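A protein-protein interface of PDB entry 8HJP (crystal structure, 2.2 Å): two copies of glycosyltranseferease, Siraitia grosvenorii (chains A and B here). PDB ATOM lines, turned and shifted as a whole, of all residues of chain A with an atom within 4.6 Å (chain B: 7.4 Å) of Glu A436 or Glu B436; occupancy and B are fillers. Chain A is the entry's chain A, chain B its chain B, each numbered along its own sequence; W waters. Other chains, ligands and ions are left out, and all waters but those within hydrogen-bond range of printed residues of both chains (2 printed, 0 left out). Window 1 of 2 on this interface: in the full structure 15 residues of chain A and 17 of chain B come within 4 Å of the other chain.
Of chain B, only Ser B32, Arg B35, Arg B36, Glu B436 and Phe B439 come within 4 Å of Glu A436.
Printed residues of chain B within 4 Å of Asp A440: Arg B35.
Glu B436 touches just these residues of chain A: Arg A35, Arg A36, Glu A436 and Phe A439.
Printed residues of chain A within 4 Å of Glu B437: Arg A35 (3.2 Å).
Of the printed residues of chain A, Phe B439 touches Glu A436 (3.3 Å).
The nearest residue of chain A that does not touch Glu B436 is Ser A32 (4.04 Å).
NH2 of Arg B36 is in hydrogen-bond range of O of Glu B436 (3.2 Å).
The backbone NH of Gly B435 lies within hydrogen-bond range of the side-chain carboxylate of Glu B437 (3.0 Å).
The backbone carbonyl oxygen (O) of Ser A32 lies within hydrogen-bond range of the guanidinium group (NH1) of Arg A36, at 3.0 Å.
The guanidinium group (NH1) of Arg B36 is in hydrogen-bond range of the backbone carbonyl oxygen (O) of Ser B32.
OE2 of Glu A437 is in hydrogen-bond range of N of Gly A435.
The guanidinium group (NH2) of Arg A36 sits at hydrogen-bond distance from the backbone carbonyl oxygen (O) of Glu A436, 3.4 Å away.
OE1 of Glu A436 is in salt-bridge range of NH1 of Arg B36 (2.7 Å).
The guanidinium group (NH2) of Arg A35 lies within salt-bridge range of the side-chain carboxylate (OD2) of Asp B440 (2.6 Å).
The guanidinium group of Arg A36 lies within salt-bridge range of the side-chain carboxylate of Glu B436 (2.7 Å).
The guanidinium group (NH2) of Arg B35 lies within salt-bridge range of the side-chain carboxylate (OD2) of Asp A440, 2.9 Å away.
Of the 17 printed residues of chain B, 7 touch a printed residue of chain A.
Hydrophobic or aromatic side chains of chain A within 4 Å of the printed part of chain B: Phe A439.
Among the printed residues, Asp or Glu carboxylates within 4 Å of a Lys or Arg side-chain nitrogen of the other chain: Arg A35 with Asp B440 (2.6 Å), Arg A36 with Glu B436 (2.7 Å), Glu A436 with Arg B36 (2.7 Å) and Asp A440 with Arg B35 (2.9 Å).
Arg A35 touches Glu B437, and with the chains exchanged Glu A437 touches Arg B35.
Glu A436 touches Ser B32, but with the chains exchanged Ser A32 does not touch Glu B436 (4.04 Å).
Glu A436 touches its own counterpart, Glu B436.
Glu A436 touches Phe B439, and with the chains exchanged Phe A439 touches Glu B436.
Positions printed for both chains: 32, 35, 36, 435, 436, 437, 438, 439 and 440.
Of the 14 pairs that touch across the chains among the printed residues, 13 have their exchanged pair printed and touching as well.
Arg B36 touches Arg A35 (CG to O, 3.4 Å).
Arg A35 touches Glu B436.
Glu B437 touches Arg A35 (CA to NH2, 3.2 Å).
Arg B35 touches Arg A36.
CA of Ser B32 touches OE1 of Glu A436, 3.9 Å away.
CB of Glu A436 touches CD of Arg B35, at 3.5 Å.
Glu A436 touches Glu B436 (CG to OE2, 3.6 Å).
Glu A436 touches Phe B439 (OE2 to CD2, 3.3 Å).
Glu A437 touches Arg B35.
Glu B436 touches Phe A439 (OE2 to CE2, 3.2 Å).
Water W1 bridges the guanidinium group of Arg B35 (2.6 Å) and the side-chain carboxylate of Glu A436 (2.8 Å).
Water W2 lies within hydrogen-bond range of the guanidinium group of Arg A35 (2.9 Å), the side-chain carboxylate of Glu B436 (2.9 Å) and the backbone NH of Ser A32 (3.4 Å).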
ATOM      1  N   SER A  32      12.955  25.842  -2.104  1.00  0.00           N
ATOM      2  CA  SER A  32      11.815  25.143  -2.686  1.00  0.00           C
ATOM      3  C   SER A  32      11.572  25.586  -4.123  1.00  0.00           C
ATOM      4  O   SER A  32      11.329  24.750  -4.997  1.00  0.00           O
ATOM      5  CB  SER A  32      10.576  25.346  -1.822  1.00  0.00           C
ATOM      6  OG  SER A  32       9.984  26.623  -2.037  1.00  0.00           O
ATOM      7  N   ARG A  35      14.192  24.125  -6.457  1.00  0.00           N
ATOM      8  CA  ARG A  35      13.925  22.717  -6.730  1.00  0.00           C
ATOM      9  C   ARG A  35      12.799  22.529  -7.738  1.00  0.00           C
ATOM     10  O   ARG A  35      12.717  21.472  -8.373  1.00  0.00           O
ATOM     11  CB  ARG A  35      13.598  21.987  -5.428  1.00  0.00           C
ATOM     12  CG  ARG A  35      14.796  21.909  -4.508  1.00  0.00           C
ATOM     13  CD  ARG A  35      14.546  21.085  -3.264  1.00  0.00           C
ATOM     14  NE  ARG A  35      15.813  20.576  -2.752  1.00  0.00           N
ATOM     15  CZ  ARG A  35      16.355  20.943  -1.597  1.00  0.00           C
ATOM     16  NH1 ARG A  35      15.732  21.814  -0.815  1.00  0.00           N
ATOM     17  NH2 ARG A  35      17.522  20.436  -1.220  1.00  0.00           N
ATOM     18  N   ARG A  36      11.926  23.523  -7.884  1.00  0.00           N
ATOM     19  CA  ARG A  36      10.806  23.478  -8.811  1.00  0.00           C
ATOM     20  C   ARG A  36      11.129  24.178 -10.128  1.00  0.00           C
ATOM     21  O   ARG A  36      10.213  24.594 -10.847  1.00  0.00           O
ATOM     22  CB  ARG A  36       9.565  24.055  -8.135  1.00  0.00           C
ATOM     23  CG  ARG A  36       9.096  23.122  -7.038  1.00  0.00           C
ATOM     24  CD  ARG A  36       8.196  23.765  -6.019  1.00  0.00           C
ATOM     25  NE  ARG A  36       7.654  22.745  -5.127  1.00  0.00           N
ATOM     26  CZ  ARG A  36       8.324  22.218  -4.108  1.00  0.00           C
ATOM     27  NH1 ARG A  36       9.572  22.601  -3.861  1.00  0.00           N
ATOM     28  NH2 ARG A  36       7.755  21.292  -3.347  1.00  0.00           N
ATOM     29  N   GLY A 435       4.565  17.259   3.640  1.00  0.00           N
ATOM     30  CA  GLY A 435       5.524  16.984   2.592  1.00  0.00           C
ATOM     31  C   GLY A 435       5.554  18.057   1.526  1.00  0.00           C
ATOM     32  O   GLY A 435       5.259  19.225   1.798  1.00  0.00           O
ATOM     33  N   GLU A 436       5.902  17.670   0.296  1.00  0.00           N
ATOM     34  CA  GLU A 436       6.081  18.638  -0.778  1.00  0.00           C
ATOM     35  C   GLU A 436       4.775  19.275  -1.236  1.00  0.00           C
ATOM     36  O   GLU A 436       4.824  20.279  -1.955  1.00  0.00           O
ATOM     37  CB  GLU A 436       6.793  17.970  -1.952  1.00  0.00           C
ATOM     38  CG  GLU A 436       8.128  17.372  -1.556  1.00  0.00           C
ATOM     39  CD  GLU A 436       8.945  16.887  -2.734  1.00  0.00           C
ATOM     40  OE1 GLU A 436       8.408  16.847  -3.861  1.00  0.00           O
ATOM     41  OE2 GLU A 436      10.129  16.536  -2.529  1.00  0.00           O
ATOM     42  N   GLU A 437       3.620  18.727  -0.842  1.00  0.00           N
ATOM     43  CA  GLU A 437       2.349  19.370  -1.166  1.00  0.00           C
ATOM     44  C   GLU A 437       2.266  20.771  -0.578  1.00  0.00           C
ATOM     45  O   GLU A 437       1.449  21.579  -1.031  1.00  0.00           O
ATOM     46  CB  GLU A 437       1.176  18.519  -0.670  1.00  0.00           C
ATOM     47  CG  GLU A 437       0.970  18.543   0.840  1.00  0.00           C
ATOM     48  CD  GLU A 437       1.982  17.685   1.581  1.00  0.00           C
ATOM     49  OE1 GLU A 437       2.764  16.977   0.915  1.00  0.00           O
ATOM     50  OE2 GLU A 437       1.993  17.718   2.830  1.00  0.00           O
ATOM     51  N   LYS A 438       3.092  21.058   0.432  1.00  0.00           N
ATOM     52  CA  LYS A 438       3.104  22.354   1.103  1.00  0.00           C
ATOM     53  C   LYS A 438       3.234  23.513   0.123  1.00  0.00           C
ATOM     54  O   LYS A 438       2.704  24.602   0.373  1.00  0.00           O
ATOM     55  CB  LYS A 438       4.247  22.378   2.124  1.00  0.00           C
ATOM     56  CG  LYS A 438       4.198  23.518   3.128  1.00  0.00           C
ATOM     57  CD  LYS A 438       5.287  23.366   4.186  1.00  0.00           C
ATOM     58  CE  LYS A 438       6.641  23.830   3.681  1.00  0.00           C
ATOM     59  NZ  LYS A 438       7.693  23.702   4.727  1.00  0.00           N
ATOM     60  N   PHE A 439       3.935  23.304  -0.990  1.00  0.00           N
ATOM     61  CA  PHE A 439       4.195  24.343  -1.979  1.00  0.00           C
ATOM     62  C   PHE A 439       3.326  24.265  -3.231  1.00  0.00           C
ATOM     63  O   PHE A 439       3.507  25.091  -4.131  1.00  0.00           O
ATOM     64  CB  PHE A 439       5.671  24.304  -2.392  1.00  0.00           C
ATOM     65  CG  PHE A 439       6.630  24.441  -1.244  1.00  0.00           C
ATOM     66  CD1 PHE A 439       6.844  25.673  -0.647  1.00  0.00           C
ATOM     67  CD2 PHE A 439       7.316  23.341  -0.759  1.00  0.00           C
ATOM     68  CE1 PHE A 439       7.728  25.806   0.407  1.00  0.00           C
ATOM     69  CE2 PHE A 439       8.202  23.467   0.296  1.00  0.00           C
ATOM     70  CZ  PHE A 439       8.407  24.703   0.879  1.00  0.00           C
ATOM     71  N   ASP A 440       2.405  23.301  -3.331  1.00  0.00           N
ATOM     72  CA  ASP A 440       1.649  23.142  -4.575  1.00  0.00           C
ATOM     73  C   ASP A 440       0.803  24.371  -4.889  1.00  0.00           C
ATOM     74  O   ASP A 440       0.788  24.849  -6.030  1.00  0.00           O
ATOM     75  CB  ASP A 440       0.761  21.898  -4.515  1.00  0.00           C
ATOM     76  CG  ASP A 440       1.552  20.618  -4.382  1.00  0.00           C
ATOM     77  OD1 ASP A 440       2.798  20.671  -4.472  1.00  0.00           O
ATOM     78  OD2 ASP A 440       0.925  19.552  -4.209  1.00  0.00           O
ATOM     79  N   GLU B  28       4.707   7.495  -5.628  1.00  0.00           N
ATOM     80  CA  GLU B  28       5.370   8.516  -4.824  1.00  0.00           C
ATOM     81  C   GLU B  28       6.513   9.169  -5.589  1.00  0.00           C
ATOM     82  O   GLU B  28       6.716  10.386  -5.493  1.00  0.00           O
ATOM     83  CB  GLU B  28       5.857   7.909  -3.510  1.00  0.00           C
ATOM     84  CG  GLU B  28       4.722   7.315  -2.692  1.00  0.00           C
ATOM     85  CD  GLU B  28       3.643   8.346  -2.397  1.00  0.00           C
ATOM     86  OE1 GLU B  28       3.987   9.433  -1.888  1.00  0.00           O
ATOM     87  OE2 GLU B  28       2.460   8.082  -2.697  1.00  0.00           O
ATOM     88  N   LYS B  31       4.995  11.628  -8.038  1.00  0.00           N
ATOM     89  CA  LYS B  31       4.618  12.907  -7.441  1.00  0.00           C
ATOM     90  C   LYS B  31       5.828  13.820  -7.282  1.00  0.00           C
ATOM     91  O   LYS B  31       5.761  15.015  -7.595  1.00  0.00           O
ATOM     92  CB  LYS B  31       3.927  12.700  -6.091  1.00  0.00           C
ATOM     93  CG  LYS B  31       2.633  11.909  -6.147  1.00  0.00           C
ATOM     94  CD  LYS B  31       2.121  11.643  -4.742  1.00  0.00           C
ATOM     95  CE  LYS B  31       0.962  10.665  -4.725  1.00  0.00           C
ATOM     96  NZ  LYS B  31       0.547  10.368  -3.326  1.00  0.00           N
ATOM     97  N   SER B  32       6.941  13.278  -6.774  1.00  0.00           N
ATOM     98  CA  SER B  32       8.160  14.071  -6.654  1.00  0.00           C
ATOM     99  C   SER B  32       8.567  14.633  -8.008  1.00  0.00           C
ATOM    100  O   SER B  32       8.919  15.812  -8.126  1.00  0.00           O
ATOM    101  CB  SER B  32       9.287  13.227  -6.059  1.00  0.00           C
ATOM    102  OG  SER B  32      10.027  12.566  -7.071  1.00  0.00           O
ATOM    103  N   LEU B  33       8.533  13.789  -9.043  1.00  0.00           N
ATOM    104  CA  LEU B  33       8.931  14.235 -10.372  1.00  0.00           C
ATOM    105  C   LEU B  33       7.967  15.290 -10.897  1.00  0.00           C
ATOM    106  O   LEU B  33       8.386  16.269 -11.525  1.00  0.00           O
ATOM    107  CB  LEU B  33       9.010  13.046 -11.327  1.00  0.00           C
ATOM    108  CG  LEU B  33      10.033  11.963 -10.963  1.00  0.00           C
ATOM    109  CD1 LEU B  33       9.798  10.712 -11.782  1.00  0.00           C
ATOM    110  CD2 LEU B  33      11.448  12.488 -11.166  1.00  0.00           C
ATOM    111  N   SER B  34       6.668  15.096 -10.662  1.00  0.00           N
ATOM    112  CA  SER B  34       5.676  16.044 -11.159  1.00  0.00           C
ATOM    113  C   SER B  34       5.895  17.426 -10.569  1.00  0.00           C
ATOM    114  O   SER B  34       5.782  18.433 -11.278  1.00  0.00           O
ATOM    115  CB  SER B  34       4.263  15.539 -10.857  1.00  0.00           C
ATOM    116  OG  SER B  34       3.343  16.615 -10.835  1.00  0.00           O
ATOM    117  N   ARG B  35       6.224  17.490  -9.276  1.00  0.00           N
ATOM    118  CA  ARG B  35       6.433  18.774  -8.628  1.00  0.00           C
ATOM    119  C   ARG B  35       7.685  19.460  -9.141  1.00  0.00           C
ATOM    120  O   ARG B  35       7.842  20.668  -8.944  1.00  0.00           O
ATOM    121  CB  ARG B  35       6.480  18.586  -7.116  1.00  0.00           C
ATOM    122  CG  ARG B  35       5.142  18.138  -6.557  1.00  0.00           C
ATOM    123  CD  ARG B  35       5.153  17.917  -5.061  1.00  0.00           C
ATOM    124  NE  ARG B  35       3.792  17.891  -4.534  1.00  0.00           N
ATOM    125  CZ  ARG B  35       3.252  16.846  -3.912  1.00  0.00           C
ATOM    126  NH1 ARG B  35       3.956  15.734  -3.731  1.00  0.00           N
ATOM    127  NH2 ARG B  35       2.002  16.910  -3.474  1.00  0.00           N
ATOM    128  N   ARG B  36       8.577  18.710  -9.788  1.00  0.00           N
ATOM    129  CA  ARG B  36       9.807  19.242 -10.348  1.00  0.00           C
ATOM    130  C   ARG B  36       9.666  19.452 -11.852  1.00  0.00           C
ATOM    131  O   ARG B  36      10.667  19.499 -12.576  1.00  0.00           O
ATOM    132  CB  ARG B  36      10.975  18.326  -9.978  1.00  0.00           C
ATOM    133  CG  ARG B  36      11.283  18.438  -8.481  1.00  0.00           C
ATOM    134  CD  ARG B  36      12.079  17.280  -7.911  1.00  0.00           C
ATOM    135  NE  ARG B  36      12.514  17.565  -6.543  1.00  0.00           N
ATOM    136  CZ  ARG B  36      11.756  17.373  -5.467  1.00  0.00           C
ATOM    137  NH1 ARG B  36      10.525  16.896  -5.596  1.00  0.00           N
ATOM    138  NH2 ARG B  36      12.225  17.656  -4.258  1.00  0.00           N
ATOM    139  N   PHE B  60      -2.994  16.600  -9.336  1.00  0.00           N
ATOM    140  CA  PHE B  60      -2.050  15.990 -10.266  1.00  0.00           C
ATOM    141  C   PHE B  60      -2.683  15.570 -11.593  1.00  0.00           C
ATOM    142  O   PHE B  60      -1.977  14.980 -12.421  1.00  0.00           O
ATOM    143  CB  PHE B  60      -1.392  14.752  -9.635  1.00  0.00           C
ATOM    144  CG  PHE B  60      -0.304  15.058  -8.630  1.00  0.00           C
ATOM    145  CD1 PHE B  60       0.954  15.462  -9.048  1.00  0.00           C
ATOM    146  CD2 PHE B  60      -0.526  14.884  -7.272  1.00  0.00           C
ATOM    147  CE1 PHE B  60       1.960  15.725  -8.131  1.00  0.00           C
ATOM    148  CE2 PHE B  60       0.479  15.142  -6.349  1.00  0.00           C
ATOM    149  CZ  PHE B  60       1.723  15.564  -6.781  1.00  0.00           C
ATOM    150  N   SER B 433      12.695  13.998   9.722  1.00  0.00           N
ATOM    151  CA  SER B 433      13.529  15.180   9.536  1.00  0.00           C
ATOM    152  C   SER B 433      13.941  15.404   8.086  1.00  0.00           C
ATOM    153  O   SER B 433      14.307  16.532   7.732  1.00  0.00           O
ATOM    154  CB  SER B 433      14.811  15.021  10.361  1.00  0.00           C
ATOM    155  OG  SER B 433      14.673  15.445  11.700  1.00  0.00           O
ATOM    156  N   LYS B 434      13.897  14.372   7.250  1.00  0.00           N
ATOM    157  CA  LYS B 434      14.337  14.515   5.870  1.00  0.00           C
ATOM    158  C   LYS B 434      13.374  15.374   5.050  1.00  0.00           C
ATOM    159  O   LYS B 434      12.149  15.306   5.211  1.00  0.00           O
ATOM    160  CB  LYS B 434      14.507  13.137   5.239  1.00  0.00           C
ATOM    161  CG  LYS B 434      15.435  12.266   6.076  1.00  0.00           C
ATOM    162  CD  LYS B 434      16.835  12.859   6.127  1.00  0.00           C
ATOM    163  CE  LYS B 434      17.795  11.975   6.913  1.00  0.00           C
ATOM    164  NZ  LYS B 434      19.226  12.322   6.658  1.00  0.00           N
ATOM    165  N   GLY B 435      13.936  16.193   4.162  1.00  0.00           N
ATOM    166  CA  GLY B 435      13.144  17.132   3.389  1.00  0.00           C
ATOM    167  C   GLY B 435      13.299  16.924   1.897  1.00  0.00           C
ATOM    168  O   GLY B 435      13.573  15.807   1.446  1.00  0.00           O
ATOM    169  N   GLU B 436      13.140  17.997   1.122  1.00  0.00           N
ATOM    170  CA  GLU B 436      13.132  17.890  -0.331  1.00  0.00           C
ATOM    171  C   GLU B 436      14.502  17.548  -0.909  1.00  0.00           C
ATOM    172  O   GLU B 436      14.583  17.171  -2.084  1.00  0.00           O
ATOM    173  CB  GLU B 436      12.567  19.178  -0.932  1.00  0.00           C
ATOM    174  CG  GLU B 436      11.186  19.499  -0.356  1.00  0.00           C
ATOM    175  CD  GLU B 436      10.422  20.558  -1.126  1.00  0.00           C
ATOM    176  OE1 GLU B 436      11.023  21.242  -1.981  1.00  0.00           O
ATOM    177  OE2 GLU B 436       9.206  20.704  -0.870  1.00  0.00           O
ATOM    178  N   GLU B 437      15.574  17.659  -0.114  1.00  0.00           N
ATOM    179  CA  GLU B 437      16.913  17.327  -0.593  1.00  0.00           C
ATOM    180  C   GLU B 437      16.995  15.876  -1.035  1.00  0.00           C
ATOM    181  O   GLU B 437      17.909  15.508  -1.780  1.00  0.00           O
ATOM    182  CB  GLU B 437      17.942  17.591   0.507  1.00  0.00           C
ATOM    183  CG  GLU B 437      17.899  16.560   1.624  1.00  0.00           C
ATOM    184  CD  GLU B 437      16.962  16.951   2.747  1.00  0.00           C
ATOM    185  OE1 GLU B 437      16.295  18.000   2.632  1.00  0.00           O
ATOM    186  OE2 GLU B 437      16.883  16.201   3.744  1.00  0.00           O
ATOM    187  N   LYS B 438      16.058  15.052  -0.561  1.00  0.00           N
ATOM    188  CA  LYS B 438      16.020  13.624  -0.850  1.00  0.00           C
ATOM    189  C   LYS B 438      16.087  13.335  -2.344  1.00  0.00           C
ATOM    190  O   LYS B 438      16.620  12.298  -2.754  1.00  0.00           O
ATOM    191  CB  LYS B 438      14.746  13.034  -0.237  1.00  0.00           C
ATOM    192  CG  LYS B 438      14.678  11.521  -0.175  1.00  0.00           C
ATOM    193  CD  LYS B 438      13.446  11.068   0.609  1.00  0.00           C
ATOM    194  CE  LYS B 438      12.176  11.120  -0.219  1.00  0.00           C
ATOM    195  NZ  LYS B 438      11.060  10.365   0.422  1.00  0.00           N
ATOM    196  N   PHE B 439      15.554  14.234  -3.169  1.00  0.00           N
ATOM    197  CA  PHE B 439      15.491  14.038  -4.611  1.00  0.00           C
ATOM    198  C   PHE B 439      16.521  14.841  -5.398  1.00  0.00           C
ATOM    199  O   PHE B 439      16.522  14.757  -6.630  1.00  0.00           O
ATOM    200  CB  PHE B 439      14.084  14.361  -5.121  1.00  0.00           C
ATOM    201  CG  PHE B 439      13.013  13.512  -4.501  1.00  0.00           C
ATOM    202  CD1 PHE B 439      12.962  12.152  -4.755  1.00  0.00           C
ATOM    203  CD2 PHE B 439      12.062  14.072  -3.665  1.00  0.00           C
ATOM    204  CE1 PHE B 439      11.984  11.363  -4.186  1.00  0.00           C
ATOM    205  CE2 PHE B 439      11.081  13.288  -3.091  1.00  0.00           C
ATOM    206  CZ  PHE B 439      11.040  11.931  -3.355  1.00  0.00           C
ATOM    207  N   ASP B 440      17.384  15.625  -4.739  1.00  0.00           N
ATOM    208  CA  ASP B 440      18.317  16.458  -5.498  1.00  0.00           C
ATOM    209  C   ASP B 440      19.240  15.604  -6.357  1.00  0.00           C
ATOM    210  O   ASP B 440      19.478  15.921  -7.529  1.00  0.00           O
ATOM    211  CB  ASP B 440      19.156  17.325  -4.555  1.00  0.00           C
ATOM    212  CG  ASP B 440      18.332  18.337  -3.789  1.00  0.00           C
ATOM    213  OD1 ASP B 440      17.141  18.514  -4.116  1.00  0.00           O
ATOM    214  OD2 ASP B 440      18.884  18.966  -2.862  1.00  0.00           O
ATOM    215  N   GLU B 441      19.776  14.520  -5.790  1.00  0.00           N
ATOM    216  CA  GLU B 441      20.742  13.709  -6.523  1.00  0.00           C
ATOM    217  C   GLU B 441      20.100  13.071  -7.749  1.00  0.00           C
ATOM    218  O   GLU B 441      20.707  13.027  -8.826  1.00  0.00           O
ATOM    219  CB  GLU B 441      21.365  12.657  -5.604  1.00  0.00           C
ATOM    220  CG  GLU B 441      22.645  12.044  -6.166  1.00  0.00           C
ATOM    221  CD  GLU B 441      23.232  10.957  -5.281  1.00  0.00           C
ATOM    222  OE1 GLU B 441      22.739  10.772  -4.150  1.00  0.00           O
ATOM    223  OE2 GLU B 441      24.198  10.294  -5.717  1.00  0.00           O
HETATM  224  O   HOH W   1       6.444  14.919  -3.687  1.00  0.00           O
HETATM  225  O   HOH W   2      13.033  22.792  -0.587  1.00  0.00           O
